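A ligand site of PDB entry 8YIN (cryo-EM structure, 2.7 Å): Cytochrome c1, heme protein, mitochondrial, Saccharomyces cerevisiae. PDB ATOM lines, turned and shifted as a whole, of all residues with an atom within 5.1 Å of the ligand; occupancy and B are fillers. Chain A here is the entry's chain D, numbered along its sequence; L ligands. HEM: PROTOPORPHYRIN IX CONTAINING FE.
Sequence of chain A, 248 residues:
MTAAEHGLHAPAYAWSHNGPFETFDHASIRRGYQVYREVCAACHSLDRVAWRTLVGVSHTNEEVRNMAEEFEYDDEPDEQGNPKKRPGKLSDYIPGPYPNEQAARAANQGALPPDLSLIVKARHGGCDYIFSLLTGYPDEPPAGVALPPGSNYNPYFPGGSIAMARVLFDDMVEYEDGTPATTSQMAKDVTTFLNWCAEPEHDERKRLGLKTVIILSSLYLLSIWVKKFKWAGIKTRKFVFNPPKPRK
OH of Tyr 129 lies within hydrogen-bond range of O1A of the ligand. The backbone NH (N) of Ala 163 sits at hydrogen-bond distance from an oxygen (O2D) of the ligand, at 2.9 Å. An oxygen (O2A) of the ligand is in salt-bridge range of the guanidinium group (NH1) of Arg 123 (3.5 Å).
The backbone carbonyl oxygen (O) of Pro 114 lies within hydrogen-bond range of a ring nitrogen (ND1) of His 44 (2.9 Å). The side-chain amide oxygen of Asn 108 sits at hydrogen-bond distance from the side-chain sulfur of Cys 43, at 3.5 Å.
A nitrogen (ND) of the ligand lies close to a ring nitrogen (NE2) of His 44. The side-chain sulfur of Met 164 lies close to a nitrogen (NA) of the ligand (3.7 Å). Val 39 touches the ligand. Cys 40 touches the ligand (CB to CAB, 3.5 Å). SG of Cys 43 touches CBC of the ligand, at 3.5 Å. Ile 119 touches the ligand. CG1 of Ile 130 touches CMA of the ligand (3.9 Å). Leu 133 touches the ligand (CD2 to CBA, 3.7 Å). Leu 134 touches the ligand. Phe 157 touches the ligand. Ile 162 touches the ligand (CG1 to O2D, 3.7 Å). CG2 of Val 167 touches CHC of the ligand, at 3.7 Å. Leu 168 touches the ligand (CD2 to CBB, 3.97 Å). 16 residues have an atom within 4 Å of the ligand: Val 39, Cys 40, Cys 43, His 44, Ile 119, Arg 123, Tyr 129, Ile 130, Leu 133, Leu 134, Phe 157, Ile 162, Ala 163, Met 164, Val 167 and Leu 168.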
ATOM      1  N   VAL A  35     -14.001   3.647 -13.509  1.00  0.00           N
ATOM      2  CA  VAL A  35     -14.914   3.213 -12.469  1.00  0.00           C
ATOM      3  C   VAL A  35     -16.156   2.562 -13.083  1.00  0.00           C
ATOM      4  O   VAL A  35     -16.876   1.823 -12.392  1.00  0.00           O
ATOM      5  CB  VAL A  35     -15.242   4.407 -11.548  1.00  0.00           C
ATOM      6  CG1 VAL A  35     -15.974   4.002 -10.278  1.00  0.00           C
ATOM      7  CG2 VAL A  35     -13.980   5.141 -11.192  1.00  0.00           C
ATOM      8  N   VAL A  39     -16.572  -1.599 -11.724  1.00  0.00           N
ATOM      9  CA  VAL A  39     -17.557  -1.534 -10.656  1.00  0.00           C
ATOM     10  C   VAL A  39     -18.973  -1.794 -11.148  1.00  0.00           C
ATOM     11  O   VAL A  39     -19.659  -2.672 -10.608  1.00  0.00           O
ATOM     12  CB  VAL A  39     -17.464  -0.184  -9.917  1.00  0.00           C
ATOM     13  CG1 VAL A  39     -18.615   0.003  -8.987  1.00  0.00           C
ATOM     14  CG2 VAL A  39     -16.156  -0.075  -9.158  1.00  0.00           C
ATOM     15  N   CYS A  40     -19.441  -1.070 -12.165  1.00  0.00           N
ATOM     16  CA  CYS A  40     -20.834  -1.193 -12.581  1.00  0.00           C
ATOM     17  C   CYS A  40     -21.008  -1.795 -13.971  1.00  0.00           C
ATOM     18  O   CYS A  40     -22.109  -1.747 -14.518  1.00  0.00           O
ATOM     19  CB  CYS A  40     -21.564   0.137 -12.529  1.00  0.00           C
ATOM     20  SG  CYS A  40     -20.698   1.539 -13.214  1.00  0.00           S
ATOM     21  N   CYS A  43     -23.454  -5.334 -13.599  1.00  0.00           N
ATOM     22  CA  CYS A  43     -24.913  -5.398 -13.577  1.00  0.00           C
ATOM     23  C   CYS A  43     -25.615  -4.338 -14.409  1.00  0.00           C
ATOM     24  O   CYS A  43     -26.787  -4.541 -14.746  1.00  0.00           O
ATOM     25  CB  CYS A  43     -25.423  -5.305 -12.130  1.00  0.00           C
ATOM     26  SG  CYS A  43     -25.506  -6.895 -11.312  1.00  0.00           S
ATOM     27  N   HIS A  44     -24.956  -3.242 -14.758  1.00  0.00           N
ATOM     28  CA  HIS A  44     -25.599  -2.186 -15.527  1.00  0.00           C
ATOM     29  C   HIS A  44     -25.103  -2.186 -16.964  1.00  0.00           C
ATOM     30  O   HIS A  44     -23.960  -2.550 -17.253  1.00  0.00           O
ATOM     31  CB  HIS A  44     -25.333  -0.826 -14.894  1.00  0.00           C
ATOM     32  CG  HIS A  44     -26.291  -0.483 -13.796  1.00  0.00           C
ATOM     33  ND1 HIS A  44     -27.644  -0.324 -14.012  1.00  0.00           N
ATOM     34  CD2 HIS A  44     -26.091  -0.267 -12.478  1.00  0.00           C
ATOM     35  CE1 HIS A  44     -28.231  -0.023 -12.868  1.00  0.00           C
ATOM     36  NE2 HIS A  44     -27.316   0.004 -11.926  1.00  0.00           N
ATOM     37  N   ASN A 108     -30.800 -10.583  -9.678  1.00  0.00           N
ATOM     38  CA  ASN A 108     -30.882  -9.370  -8.877  1.00  0.00           C
ATOM     39  C   ASN A 108     -32.079  -9.380  -7.932  1.00  0.00           C
ATOM     40  O   ASN A 108     -32.484  -8.318  -7.446  1.00  0.00           O
ATOM     41  CB  ASN A 108     -30.949  -8.128  -9.772  1.00  0.00           C
ATOM     42  CG  ASN A 108     -29.678  -7.925 -10.569  1.00  0.00           C
ATOM     43  OD1 ASN A 108     -28.641  -7.558 -10.008  1.00  0.00           O
ATOM     44  ND2 ASN A 108     -29.744  -8.161 -11.871  1.00  0.00           N
ATOM     45  N   ALA A 111     -35.633  -7.464  -9.065  1.00  0.00           N
ATOM     46  CA  ALA A 111     -35.464  -6.144  -9.654  1.00  0.00           C
ATOM     47  C   ALA A 111     -34.815  -6.243 -11.026  1.00  0.00           C
ATOM     48  O   ALA A 111     -34.275  -7.280 -11.415  1.00  0.00           O
ATOM     49  CB  ALA A 111     -34.640  -5.252  -8.733  1.00  0.00           C
ATOM     50  N   LEU A 112     -34.872  -5.147 -11.765  1.00  0.00           N
ATOM     51  CA  LEU A 112     -34.217  -5.035 -13.067  1.00  0.00           C
ATOM     52  C   LEU A 112     -33.407  -3.758 -13.072  1.00  0.00           C
ATOM     53  O   LEU A 112     -33.998  -2.655 -12.988  1.00  0.00           O
ATOM     54  CB  LEU A 112     -35.236  -5.042 -14.211  1.00  0.00           C
ATOM     55  CG  LEU A 112     -34.722  -4.745 -15.616  1.00  0.00           C
ATOM     56  CD1 LEU A 112     -33.859  -5.870 -16.131  1.00  0.00           C
ATOM     57  CD2 LEU A 112     -35.875  -4.503 -16.563  1.00  0.00           C
ATOM     58  N   PRO A 113     -32.083  -3.828 -13.133  1.00  0.00           N
ATOM     59  CA  PRO A 113     -31.271  -2.623 -13.199  1.00  0.00           C
ATOM     60  C   PRO A 113     -31.402  -1.960 -14.561  1.00  0.00           C
ATOM     61  O   PRO A 113     -31.299  -2.626 -15.603  1.00  0.00           O
ATOM     62  CB  PRO A 113     -29.847  -3.142 -12.960  1.00  0.00           C
ATOM     63  CG  PRO A 113     -29.880  -4.552 -13.331  1.00  0.00           C
ATOM     64  CD  PRO A 113     -31.251  -5.042 -13.029  1.00  0.00           C
ATOM     65  N   PRO A 114     -31.625  -0.659 -14.606  1.00  0.00           N
ATOM     66  CA  PRO A 114     -31.919   0.019 -15.870  1.00  0.00           C
ATOM     67  C   PRO A 114     -30.650   0.292 -16.669  1.00  0.00           C
ATOM     68  O   PRO A 114     -29.528   0.000 -16.251  1.00  0.00           O
ATOM     69  CB  PRO A 114     -32.571   1.324 -15.416  1.00  0.00           C
ATOM     70  CG  PRO A 114     -31.927   1.612 -14.131  1.00  0.00           C
ATOM     71  CD  PRO A 114     -31.677   0.287 -13.469  1.00  0.00           C
ATOM     72  N   LEU A 116     -27.923   2.873 -18.236  1.00  0.00           N
ATOM     73  CA  LEU A 116     -27.304   4.085 -17.716  1.00  0.00           C
ATOM     74  C   LEU A 116     -26.856   5.033 -18.812  1.00  0.00           C
ATOM     75  O   LEU A 116     -25.967   5.856 -18.592  1.00  0.00           O
ATOM     76  CB  LEU A 116     -26.133   3.740 -16.806  1.00  0.00           C
ATOM     77  CG  LEU A 116     -26.434   2.996 -15.511  1.00  0.00           C
ATOM     78  CD1 LEU A 116     -25.233   3.033 -14.584  1.00  0.00           C
ATOM     79  CD2 LEU A 116     -27.665   3.551 -14.809  1.00  0.00           C
ATOM     80  N   ILE A 119     -29.518   8.811 -17.983  1.00  0.00           N
ATOM     81  CA  ILE A 119     -29.881   8.725 -16.574  1.00  0.00           C
ATOM     82  C   ILE A 119     -29.725  10.040 -15.825  1.00  0.00           C
ATOM     83  O   ILE A 119     -30.435  10.268 -14.823  1.00  0.00           O
ATOM     84  CB  ILE A 119     -29.074   7.584 -15.901  1.00  0.00           C
ATOM     85  CG1 ILE A 119     -29.661   7.185 -14.538  1.00  0.00           C
ATOM     86  CG2 ILE A 119     -27.600   7.909 -15.826  1.00  0.00           C
ATOM     87  CD1 ILE A 119     -30.990   6.507 -14.636  1.00  0.00           C
ATOM     88  N   ARG A 123     -33.978  11.808 -14.917  1.00  0.00           N
ATOM     89  CA  ARG A 123     -34.239  11.852 -13.493  1.00  0.00           C
ATOM     90  C   ARG A 123     -34.348  13.302 -13.050  1.00  0.00           C
ATOM     91  O   ARG A 123     -33.643  14.166 -13.560  1.00  0.00           O
ATOM     92  CB  ARG A 123     -33.134  11.146 -12.687  1.00  0.00           C
ATOM     93  CG  ARG A 123     -33.106   9.628 -12.811  1.00  0.00           C
ATOM     94  CD  ARG A 123     -34.397   8.988 -12.331  1.00  0.00           C
ATOM     95  NE  ARG A 123     -34.459   7.552 -12.581  1.00  0.00           N
ATOM     96  CZ  ARG A 123     -34.815   7.009 -13.740  1.00  0.00           C
ATOM     97  NH1 ARG A 123     -34.855   5.690 -13.876  1.00  0.00           N
ATOM     98  NH2 ARG A 123     -35.142   7.764 -14.768  1.00  0.00           N
ATOM     99  N   TYR A 129     -28.422  14.275  -8.707  1.00  0.00           N
ATOM    100  CA  TYR A 129     -29.119  13.107  -8.191  1.00  0.00           C
ATOM    101  C   TYR A 129     -28.194  11.908  -8.110  1.00  0.00           C
ATOM    102  O   TYR A 129     -28.174  11.205  -7.090  1.00  0.00           O
ATOM    103  CB  TYR A 129     -30.339  12.778  -9.046  1.00  0.00           C
ATOM    104  CG  TYR A 129     -31.165  11.645  -8.486  1.00  0.00           C
ATOM    105  CD1 TYR A 129     -31.609  11.672  -7.167  1.00  0.00           C
ATOM    106  CD2 TYR A 129     -31.508  10.542  -9.268  1.00  0.00           C
ATOM    107  CE1 TYR A 129     -32.357  10.648  -6.642  1.00  0.00           C
ATOM    108  CE2 TYR A 129     -32.261   9.506  -8.739  1.00  0.00           C
ATOM    109  CZ  TYR A 129     -32.677   9.565  -7.438  1.00  0.00           C
ATOM    110  OH  TYR A 129     -33.428   8.548  -6.894  1.00  0.00           O
ATOM    111  N   ILE A 130     -27.421  11.643  -9.164  1.00  0.00           N
ATOM    112  CA  ILE A 130     -26.458  10.544  -9.089  1.00  0.00           C
ATOM    113  C   ILE A 130     -25.133  11.116  -8.596  1.00  0.00           C
ATOM    114  O   ILE A 130     -24.126  11.135  -9.307  1.00  0.00           O
ATOM    115  CB  ILE A 130     -26.310   9.907 -10.474  1.00  0.00           C
ATOM    116  CG1 ILE A 130     -27.684   9.715 -11.088  1.00  0.00           C
ATOM    117  CG2 ILE A 130     -25.685   8.546 -10.382  1.00  0.00           C
ATOM    118  CD1 ILE A 130     -27.641   9.524 -12.538  1.00  0.00           C
ATOM    119  N   LEU A 133     -27.278   9.708  -4.418  1.00  0.00           N
ATOM    120  CA  LEU A 133     -27.736   8.332  -4.458  1.00  0.00           C
ATOM    121  C   LEU A 133     -26.605   7.381  -4.056  1.00  0.00           C
ATOM    122  O   LEU A 133     -26.813   6.454  -3.272  1.00  0.00           O
ATOM    123  CB  LEU A 133     -28.250   8.004  -5.859  1.00  0.00           C
ATOM    124  CG  LEU A 133     -28.819   6.615  -6.144  1.00  0.00           C
ATOM    125  CD1 LEU A 133     -30.100   6.388  -5.363  1.00  0.00           C
ATOM    126  CD2 LEU A 133     -29.082   6.473  -7.612  1.00  0.00           C
ATOM    127  N   LEU A 134     -25.404   7.623  -4.578  1.00  0.00           N
ATOM    128  CA  LEU A 134     -24.279   6.744  -4.286  1.00  0.00           C
ATOM    129  C   LEU A 134     -23.653   7.071  -2.942  1.00  0.00           C
ATOM    130  O   LEU A 134     -23.322   6.165  -2.172  1.00  0.00           O
ATOM    131  CB  LEU A 134     -23.243   6.866  -5.398  1.00  0.00           C
ATOM    132  CG  LEU A 134     -23.849   6.762  -6.779  1.00  0.00           C
ATOM    133  CD1 LEU A 134     -22.809   7.123  -7.809  1.00  0.00           C
ATOM    134  CD2 LEU A 134     -24.395   5.375  -7.030  1.00  0.00           C
ATOM    135  N   PHE A 157     -34.056   7.689  -3.207  1.00  0.00           N
ATOM    136  CA  PHE A 157     -35.018   6.964  -4.012  1.00  0.00           C
ATOM    137  C   PHE A 157     -36.419   7.252  -3.459  1.00  0.00           C
ATOM    138  O   PHE A 157     -36.602   7.310  -2.251  1.00  0.00           O
ATOM    139  CB  PHE A 157     -34.721   5.476  -3.959  1.00  0.00           C
ATOM    140  CG  PHE A 157     -35.273   4.702  -5.113  1.00  0.00           C
ATOM    141  CD1 PHE A 157     -34.896   5.008  -6.412  1.00  0.00           C
ATOM    142  CD2 PHE A 157     -36.136   3.649  -4.902  1.00  0.00           C
ATOM    143  CE1 PHE A 157     -35.400   4.299  -7.463  1.00  0.00           C
ATOM    144  CE2 PHE A 157     -36.639   2.937  -5.963  1.00  0.00           C
ATOM    145  CZ  PHE A 157     -36.268   3.257  -7.247  1.00  0.00           C
ATOM    146  N   ILE A 162     -34.668   0.828  -1.681  1.00  0.00           N
ATOM    147  CA  ILE A 162     -34.094   0.614  -3.005  1.00  0.00           C
ATOM    148  C   ILE A 162     -33.415  -0.747  -3.012  1.00  0.00           C
ATOM    149  O   ILE A 162     -32.832  -1.168  -2.014  1.00  0.00           O
ATOM    150  CB  ILE A 162     -33.119   1.771  -3.371  1.00  0.00           C
ATOM    151  CG1 ILE A 162     -32.464   1.570  -4.740  1.00  0.00           C
ATOM    152  CG2 ILE A 162     -32.074   1.988  -2.303  1.00  0.00           C
ATOM    153  CD1 ILE A 162     -31.679   2.766  -5.210  1.00  0.00           C
ATOM    154  N   ALA A 163     -33.548  -1.461  -4.136  1.00  0.00           N
ATOM    155  CA  ALA A 163     -32.944  -2.789  -4.260  1.00  0.00           C
ATOM    156  C   ALA A 163     -31.428  -2.731  -4.368  1.00  0.00           C
ATOM    157  O   ALA A 163     -30.769  -3.731  -4.104  1.00  0.00           O
ATOM    158  CB  ALA A 163     -33.527  -3.505  -5.470  1.00  0.00           C
ATOM    159  N   MET A 164     -30.866  -1.578  -4.750  1.00  0.00           N
ATOM    160  CA  MET A 164     -29.435  -1.446  -4.979  1.00  0.00           C
ATOM    161  C   MET A 164     -28.673  -1.299  -3.663  1.00  0.00           C
ATOM    162  O   MET A 164     -29.049  -0.500  -2.801  1.00  0.00           O
ATOM    163  CB  MET A 164     -29.178  -0.223  -5.864  1.00  0.00           C
ATOM    164  CG  MET A 164     -27.727   0.089  -6.117  1.00  0.00           C
ATOM    165  SD  MET A 164     -27.461   1.827  -6.447  1.00  0.00           S
ATOM    166  CE  MET A 164     -25.677   1.870  -6.490  1.00  0.00           C
ATOM    167  N   VAL A 167     -21.993   0.136  -3.411  1.00  0.00           N
ATOM    168  CA  VAL A 167     -20.899  -0.504  -4.116  1.00  0.00           C
ATOM    169  C   VAL A 167     -19.576   0.234  -3.922  1.00  0.00           C
ATOM    170  O   VAL A 167     -18.523  -0.401  -3.879  1.00  0.00           O
ATOM    171  CB  VAL A 167     -21.217  -0.649  -5.612  1.00  0.00           C
ATOM    172  CG1 VAL A 167     -20.331  -1.691  -6.247  1.00  0.00           C
ATOM    173  CG2 VAL A 167     -22.669  -1.002  -5.813  1.00  0.00           C
ATOM    174  N   LEU A 168     -19.612   1.550  -3.753  1.00  0.00           N
ATOM    175  CA  LEU A 168     -18.391   2.353  -3.681  1.00  0.00           C
ATOM    176  C   LEU A 168     -17.851   2.322  -2.254  1.00  0.00           C
ATOM    177  O   LEU A 168     -18.554   2.688  -1.307  1.00  0.00           O
ATOM    178  CB  LEU A 168     -18.650   3.794  -4.106  1.00  0.00           C
ATOM    179  CG  LEU A 168     -19.095   4.056  -5.553  1.00  0.00           C
ATOM    180  CD1 LEU A 168     -18.936   5.520  -5.862  1.00  0.00           C
ATOM    181  CD2 LEU A 168     -18.321   3.218  -6.547  1.00  0.00           C
ATOM    182  N   VAL A 190     -17.744   9.184 -12.002  1.00  0.00           N
ATOM    183  CA  VAL A 190     -18.789   8.472 -12.727  1.00  0.00           C
ATOM    184  C   VAL A 190     -19.855   9.447 -13.212  1.00  0.00           C
ATOM    185  O   VAL A 190     -20.378   9.302 -14.324  1.00  0.00           O
ATOM    186  CB  VAL A 190     -19.409   7.344 -11.883  1.00  0.00           C
ATOM    187  CG1 VAL A 190     -18.525   6.154 -11.875  1.00  0.00           C
ATOM    188  CG2 VAL A 190     -19.686   7.795 -10.468  1.00  0.00           C
ATOM    189  N   LEU A 194     -20.977   9.952 -16.898  1.00  0.00           N
ATOM    190  CA  LEU A 194     -22.344   9.625 -17.264  1.00  0.00           C
ATOM    191  C   LEU A 194     -23.094  10.812 -17.837  1.00  0.00           C
ATOM    192  O   LEU A 194     -23.971  10.625 -18.689  1.00  0.00           O
ATOM    193  CB  LEU A 194     -23.102   9.070 -16.066  1.00  0.00           C
ATOM    194  CG  LEU A 194     -22.831   7.599 -15.735  1.00  0.00           C
ATOM    195  CD1 LEU A 194     -23.608   7.196 -14.494  1.00  0.00           C
ATOM    196  CD2 LEU A 194     -23.165   6.683 -16.896  1.00  0.00           C
HETATM  197  CHA HEM L   1     -30.183   1.366  -9.857  1.00  0.00           C
HETATM  198  CHB HEM L   1     -26.093   3.838 -10.596  1.00  0.00           C
HETATM  199  CHC HEM L   1     -23.484  -0.008  -9.274  1.00  0.00           C
HETATM  200  CHD HEM L   1     -27.581  -2.542  -8.739  1.00  0.00           C
HETATM  201  C1A HEM L   1     -29.303   2.381 -10.158  1.00  0.00           C
HETATM  202  C2A HEM L   1     -29.653   3.714 -10.582  1.00  0.00           C
HETATM  203  C3A HEM L   1     -28.526   4.381 -10.787  1.00  0.00           C
HETATM  204  C4A HEM L   1     -27.423   3.501 -10.498  1.00  0.00           C
HETATM  205  CMA HEM L   1     -28.427   5.846 -11.253  1.00  0.00           C
HETATM  206  CAA HEM L   1     -31.078   4.259 -10.787  1.00  0.00           C
HETATM  207  CBA HEM L   1     -31.726   4.643  -9.477  1.00  0.00           C
HETATM  208  CGA HEM L   1     -33.074   5.206  -9.825  1.00  0.00           C
HETATM  209  O1A HEM L   1     -33.485   6.198  -9.180  1.00  0.00           O
HETATM  210  O2A HEM L   1     -33.722   4.676 -10.754  1.00  0.00           O
HETATM  211  C1B HEM L   1     -25.040   3.015 -10.279  1.00  0.00           C
HETATM  212  C2B HEM L   1     -23.661   3.414 -10.285  1.00  0.00           C
HETATM  213  C3B HEM L   1     -22.915   2.358  -9.915  1.00  0.00           C
HETATM  214  C4B HEM L   1     -23.827   1.269  -9.669  1.00  0.00           C
HETATM  215  CMB HEM L   1     -23.282   4.859 -10.683  1.00  0.00           C
HETATM  216  CAB HEM L   1     -21.382   2.173  -9.728  1.00  0.00           C
HETATM  217  CBB HEM L   1     -20.398   3.055  -9.928  1.00  0.00           C
HETATM  218  C1C HEM L   1     -24.374  -1.053  -9.092  1.00  0.00           C
HETATM  219  C2C HEM L   1     -24.012  -2.444  -8.944  1.00  0.00           C
HETATM  220  C3C HEM L   1     -25.165  -3.150  -8.805  1.00  0.00           C
HETATM  221  C4C HEM L   1     -26.254  -2.200  -8.850  1.00  0.00           C
HETATM  222  CMC HEM L   1     -22.557  -2.926  -8.979  1.00  0.00           C
HETATM  223  CAC HEM L   1     -25.449  -4.659  -8.595  1.00  0.00           C
HETATM  224  CBC HEM L   1     -24.609  -5.612  -8.182  1.00  0.00           C
HETATM  225  C1D HEM L   1     -28.647  -1.713  -8.995  1.00  0.00           C
HETATM  226  C2D HEM L   1     -30.044  -2.073  -8.899  1.00  0.00           C
HETATM  227  C3D HEM L   1     -30.758  -0.989  -9.209  1.00  0.00           C
HETATM  228  C4D HEM L   1     -29.839   0.084  -9.503  1.00  0.00           C
HETATM  229  CMD HEM L   1     -30.599  -3.459  -8.513  1.00  0.00           C
HETATM  230  CAD HEM L   1     -32.299  -0.893  -9.251  1.00  0.00           C
HETATM  231  CBD HEM L   1     -32.822  -0.163  -8.016  1.00  0.00           C
HETATM  232  CGD HEM L   1     -34.277  -0.472  -7.838  1.00  0.00           C
HETATM  233  O1D HEM L   1     -34.984  -0.559  -8.868  1.00  0.00           O
HETATM  234  O2D HEM L   1     -34.725  -0.621  -6.685  1.00  0.00           O
HETATM  235  NA  HEM L   1     -27.925   2.277 -10.105  1.00  0.00           N
HETATM  236  NB  HEM L   1     -25.122   1.691  -9.899  1.00  0.00           N
HETATM  237  NC  HEM L   1     -25.745  -0.935  -9.032  1.00  0.00           N
HETATM  238  ND  HEM L   1     -28.554  -0.387  -9.353  1.00  0.00           N
HETATM  239 FE   HEM L   1     -26.854   0.730  -9.293  1.00  0.00          FE
